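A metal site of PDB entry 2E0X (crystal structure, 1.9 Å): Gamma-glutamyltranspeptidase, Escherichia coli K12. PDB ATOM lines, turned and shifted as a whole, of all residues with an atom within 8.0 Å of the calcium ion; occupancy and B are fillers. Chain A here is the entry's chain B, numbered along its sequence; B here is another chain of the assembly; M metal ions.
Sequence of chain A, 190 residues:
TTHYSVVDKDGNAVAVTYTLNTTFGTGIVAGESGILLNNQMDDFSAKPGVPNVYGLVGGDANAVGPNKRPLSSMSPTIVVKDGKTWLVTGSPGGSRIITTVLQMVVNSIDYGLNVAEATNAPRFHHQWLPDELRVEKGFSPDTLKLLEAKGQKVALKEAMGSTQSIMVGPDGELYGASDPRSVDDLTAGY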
ATOM      1  N   THR A 119     -33.333 -16.132  19.022  1.00  0.00           N
ATOM      2  CA  THR A 119     -32.850 -17.473  19.419  1.00  0.00           C
ATOM      3  C   THR A 119     -31.908 -17.428  20.633  1.00  0.00           C
ATOM      4  O   THR A 119     -32.025 -18.254  21.551  1.00  0.00           O
ATOM      5  CB  THR A 119     -32.130 -18.122  18.209  1.00  0.00           C
ATOM      6  OG1 THR A 119     -33.103 -18.452  17.214  1.00  0.00           O
ATOM      7  CG2 THR A 119     -31.388 -19.382  18.586  1.00  0.00           C
ATOM      8  N   ASN A 120     -30.987 -16.478  20.615  1.00  0.00           N
ATOM      9  CA  ASN A 120     -29.977 -16.317  21.663  1.00  0.00           C
ATOM     10  C   ASN A 120     -30.465 -15.557  22.899  1.00  0.00           C
ATOM     11  O   ASN A 120     -29.797 -15.585  23.946  1.00  0.00           O
ATOM     12  CB  ASN A 120     -28.707 -15.681  21.088  1.00  0.00           C
ATOM     13  CG  ASN A 120     -27.927 -16.624  20.180  1.00  0.00           C
ATOM     14  OD1 ASN A 120     -27.062 -17.357  20.647  1.00  0.00           O
ATOM     15  ND2 ASN A 120     -28.270 -16.653  18.896  1.00  0.00           N
ATOM     16  N   SER A 162     -34.098 -26.137  22.284  1.00  0.00           N
ATOM     17  CA  SER A 162     -33.107 -26.142  21.208  1.00  0.00           C
ATOM     18  C   SER A 162     -33.878 -25.758  19.952  1.00  0.00           C
ATOM     19  O   SER A 162     -34.303 -26.629  19.191  1.00  0.00           O
ATOM     20  CB  SER A 162     -32.429 -27.505  21.057  1.00  0.00           C
ATOM     21  OG  SER A 162     -31.565 -27.502  19.922  1.00  0.00           O
ATOM     22  N   THR A 163     -34.089 -24.460  19.764  1.00  0.00           N
ATOM     23  CA  THR A 163     -34.825 -23.986  18.591  1.00  0.00           C
ATOM     24  C   THR A 163     -33.950 -24.105  17.355  1.00  0.00           C
ATOM     25  O   THR A 163     -32.743 -23.845  17.405  1.00  0.00           O
ATOM     26  CB  THR A 163     -35.256 -22.512  18.733  1.00  0.00           C
ATOM     27  OG1 THR A 163     -34.105 -21.745  19.082  1.00  0.00           O
ATOM     28  CG2 THR A 163     -36.297 -22.359  19.809  1.00  0.00           C
ATOM     29  N   GLN A 164     -34.568 -24.476  16.240  1.00  0.00           N
ATOM     30  CA  GLN A 164     -33.850 -24.561  14.977  1.00  0.00           C
ATOM     31  C   GLN A 164     -34.804 -23.943  14.006  1.00  0.00           C
ATOM     32  O   GLN A 164     -35.836 -24.545  13.662  1.00  0.00           O
ATOM     33  CB  GLN A 164     -33.534 -26.010  14.596  1.00  0.00           C
ATOM     34  CG  GLN A 164     -32.790 -26.822  15.669  1.00  0.00           C
ATOM     35  CD  GLN A 164     -31.356 -26.346  15.878  1.00  0.00           C
ATOM     36  OE1 GLN A 164     -30.728 -25.835  14.961  1.00  0.00           O
ATOM     37  NE2 GLN A 164     -30.830 -26.556  17.081  1.00  0.00           N
ATOM     38  N   ALA A 177     -31.161 -19.668  12.369  1.00  0.00           N
ATOM     39  CA  ALA A 177     -30.482 -19.690  13.659  1.00  0.00           C
ATOM     40  C   ALA A 177     -30.654 -21.028  14.340  1.00  0.00           C
ATOM     41  O   ALA A 177     -31.765 -21.550  14.455  1.00  0.00           O
ATOM     42  CB  ALA A 177     -31.003 -18.570  14.578  1.00  0.00           C
ATOM     43  N   SER A 178     -29.518 -21.598  14.749  1.00  0.00           N
ATOM     44  CA  SER A 178     -29.454 -22.744  15.614  1.00  0.00           C
ATOM     45  C   SER A 178     -29.251 -22.264  17.044  1.00  0.00           C
ATOM     46  O   SER A 178     -28.596 -21.234  17.302  1.00  0.00           O
ATOM     47  CB  SER A 178     -28.280 -23.649  15.194  1.00  0.00           C
ATOM     48  OG  SER A 178     -28.655 -24.447  14.080  1.00  0.00           O
ATOM     49  N   ASP A 179     -29.806 -23.010  17.990  1.00  0.00           N
ATOM     50  CA  ASP A 179     -29.775 -22.635  19.393  1.00  0.00           C
ATOM     51  C   ASP A 179     -28.350 -22.657  19.933  1.00  0.00           C
ATOM     52  O   ASP A 179     -27.604 -23.623  19.670  1.00  0.00           O
ATOM     53  CB  ASP A 179     -30.671 -23.582  20.221  1.00  0.00           C
ATOM     54  CG  ASP A 179     -31.255 -22.914  21.444  1.00  0.00           C
ATOM     55  OD1 ASP A 179     -32.487 -22.967  21.629  1.00  0.00           O
ATOM     56  OD2 ASP A 179     -30.479 -22.306  22.221  1.00  0.00           O
ATOM     57  N   PRO A 180     -27.940 -21.626  20.690  1.00  0.00           N
ATOM     58  CA  PRO A 180     -26.646 -21.773  21.384  1.00  0.00           C
ATOM     59  C   PRO A 180     -26.654 -22.899  22.436  1.00  0.00           C
ATOM     60  O   PRO A 180     -25.602 -23.410  22.794  1.00  0.00           O
ATOM     61  CB  PRO A 180     -26.454 -20.434  22.072  1.00  0.00           C
ATOM     62  CG  PRO A 180     -27.831 -19.862  22.205  1.00  0.00           C
ATOM     63  CD  PRO A 180     -28.560 -20.311  20.957  1.00  0.00           C
ATOM     64  N   ARG A 181     -27.846 -23.290  22.909  1.00  0.00           N
ATOM     65  CA  ARG A 181     -27.953 -24.273  24.012  1.00  0.00           C
ATOM     66  C   ARG A 181     -27.557 -25.690  23.603  1.00  0.00           C
ATOM     67  O   ARG A 181     -27.322 -26.543  24.458  1.00  0.00           O
ATOM     68  CB  ARG A 181     -29.362 -24.259  24.602  1.00  0.00           C
ATOM     69  CG  ARG A 181     -29.733 -22.929  25.259  1.00  0.00           C
ATOM     70  CD  ARG A 181     -31.222 -22.708  25.197  1.00  0.00           C
ATOM     71  NE  ARG A 181     -31.625 -21.381  25.668  1.00  0.00           N
ATOM     72  CZ  ARG A 181     -31.694 -20.292  24.908  1.00  0.00           C
ATOM     73  NH1 ARG A 181     -31.365 -20.345  23.627  1.00  0.00           N
ATOM     74  NH2 ARG A 181     -32.094 -19.131  25.440  1.00  0.00           N
ATOM     75  N   SER A 182     -27.486 -25.928  22.291  1.00  0.00           N
ATOM     76  CA  SER A 182     -27.102 -27.227  21.729  1.00  0.00           C
ATOM     77  C   SER A 182     -25.777 -27.100  20.999  1.00  0.00           C
ATOM     78  O   SER A 182     -25.666 -26.333  20.059  1.00  0.00           O
ATOM     79  CB  SER A 182     -28.176 -27.733  20.735  1.00  0.00           C
ATOM     80  OG  SER A 182     -29.276 -28.295  21.419  1.00  0.00           O
ATOM     81  N   VAL A 183     -24.759 -27.834  21.434  1.00  0.00           N
ATOM     82  CA  VAL A 183     -23.479 -27.881  20.691  1.00  0.00           C
ATOM     83  C   VAL A 183     -23.591 -28.810  19.487  1.00  0.00           C
ATOM     84  O   VAL A 183     -24.409 -29.733  19.479  1.00  0.00           O
ATOM     85  CB  VAL A 183     -22.274 -28.304  21.580  1.00  0.00           C
ATOM     86  CG1 VAL A 183     -22.115 -27.351  22.773  1.00  0.00           C
ATOM     87  CG2 VAL A 183     -22.417 -29.746  22.052  1.00  0.00           C
ATOM     88  N   ASP A 184     -22.747 -28.541  18.482  1.00  0.00           N
ATOM     89  CA  ASP A 184     -22.563 -29.370  17.274  1.00  0.00           C
ATOM     90  C   ASP A 184     -23.741 -29.341  16.315  1.00  0.00           C
ATOM     91  O   ASP A 184     -23.827 -30.160  15.400  1.00  0.00           O
ATOM     92  CB  ASP A 184     -22.159 -30.822  17.613  1.00  0.00           C
ATOM     93  CG  ASP A 184     -20.776 -30.926  18.260  1.00  0.00           C
ATOM     94  OD1 ASP A 184     -19.840 -30.266  17.774  1.00  0.00           O
ATOM     95  OD2 ASP A 184     -20.612 -31.696  19.233  1.00  0.00           O
ATOM     96  N   ASP A 185     -24.666 -28.400  16.534  1.00  0.00           N
ATOM     97  CA  ASP A 185     -25.817 -28.210  15.649  1.00  0.00           C
ATOM     98  C   ASP A 185     -25.428 -27.284  14.501  1.00  0.00           C
ATOM     99  O   ASP A 185     -24.338 -26.708  14.498  1.00  0.00           O
ATOM    100  CB  ASP A 185     -27.043 -27.680  16.413  1.00  0.00           C
ATOM    101  CG  ASP A 185     -26.806 -26.378  17.127  1.00  0.00           C
ATOM    102  OD1 ASP A 185     -25.668 -25.839  17.068  1.00  0.00           O
ATOM    103  OD2 ASP A 185     -27.743 -25.868  17.760  1.00  0.00           O
ATOM    104  N   LEU A 186     -26.322 -27.155  13.518  1.00  0.00           N
ATOM    105  CA  LEU A 186     -26.015 -26.370  12.335  1.00  0.00           C
ATOM    106  C   LEU A 186     -27.266 -25.903  11.612  1.00  0.00           C
ATOM    107  O   LEU A 186     -28.214 -26.671  11.413  1.00  0.00           O
ATOM    108  CB  LEU A 186     -25.137 -27.167  11.351  1.00  0.00           C
ATOM    109  CG  LEU A 186     -24.512 -26.429  10.148  1.00  0.00           C
ATOM    110  CD1 LEU A 186     -23.544 -25.372  10.632  1.00  0.00           C
ATOM    111  CD2 LEU A 186     -23.808 -27.428   9.220  1.00  0.00           C
ATOM    112  N   THR A 187     -27.252 -24.642  11.202  1.00  0.00           N
ATOM    113  CA  THR A 187     -28.159 -24.118  10.196  1.00  0.00           C
ATOM    114  C   THR A 187     -27.307 -23.748   8.977  1.00  0.00           C
ATOM    115  O   THR A 187     -26.294 -23.052   9.101  1.00  0.00           O
ATOM    116  CB  THR A 187     -28.943 -22.888  10.736  1.00  0.00           C
ATOM    117  OG1 THR A 187     -29.725 -23.289  11.862  1.00  0.00           O
ATOM    118  CG2 THR A 187     -29.890 -22.333   9.696  1.00  0.00           C
ATOM    119  N   SER B  29     -30.972 -27.772  12.098  1.00  0.00           N
ATOM    120  CA  SER B  29     -31.158 -29.002  12.875  1.00  0.00           C
ATOM    121  C   SER B  29     -30.111 -29.078  13.978  1.00  0.00           C
ATOM    122  O   SER B  29     -29.143 -28.305  13.983  1.00  0.00           O
ATOM    123  CB  SER B  29     -31.149 -30.262  11.997  1.00  0.00           C
ATOM    124  OG  SER B  29     -29.859 -30.854  11.906  1.00  0.00           O
ATOM    125  N   VAL B  30     -30.322 -30.016  14.903  1.00  0.00           N
ATOM    126  CA  VAL B  30     -29.459 -30.218  16.061  1.00  0.00           C
ATOM    127  C   VAL B  30     -28.106 -30.844  15.677  1.00  0.00           C
ATOM    128  O   VAL B  30     -27.182 -30.880  16.495  1.00  0.00           O
ATOM    129  CB  VAL B  30     -30.193 -31.141  17.111  1.00  0.00           C
ATOM    130  CG1 VAL B  30     -30.106 -32.595  16.671  1.00  0.00           C
ATOM    131  CG2 VAL B  30     -29.619 -30.946  18.543  1.00  0.00           C
HETATM  132 CA    CA M   1     -25.627 -24.377  18.726  1.00  0.00          CA
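OG of Ser 182 sits at hydrogen-bond distance from OG of Ser 162 (2.8 Å).
OD2 of Asp 179 lies within salt-bridge range of NH1 of Arg 181 (2.6 Å).
OD1 of Asp 179 lies within hydrogen-bond range of N of Thr 163 (2.9 Å).
The side-chain amide nitrogen (NE2) of Gln 164 lies close to the side-chain carboxylate (OD2) of Asp 185 (3.2 Å).
CA of Pro 180 touches the calcium ion, at 3.9 Å.
Four residues have an atom within 4 Å of the calcium ion: Asp 179, Pro 180, Ser 182 and Asp 185.
The calcium ion is bound by the side-chain carboxylate (OD1) of Asp 185, the backbone carbonyl oxygen (O) of Asp 179, the backbone carbonyl oxygen (O) of Ser 182 and the side-chain carboxylate (OD2) of Asp 185.
The calcium ion has four donor atoms within binding distance.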
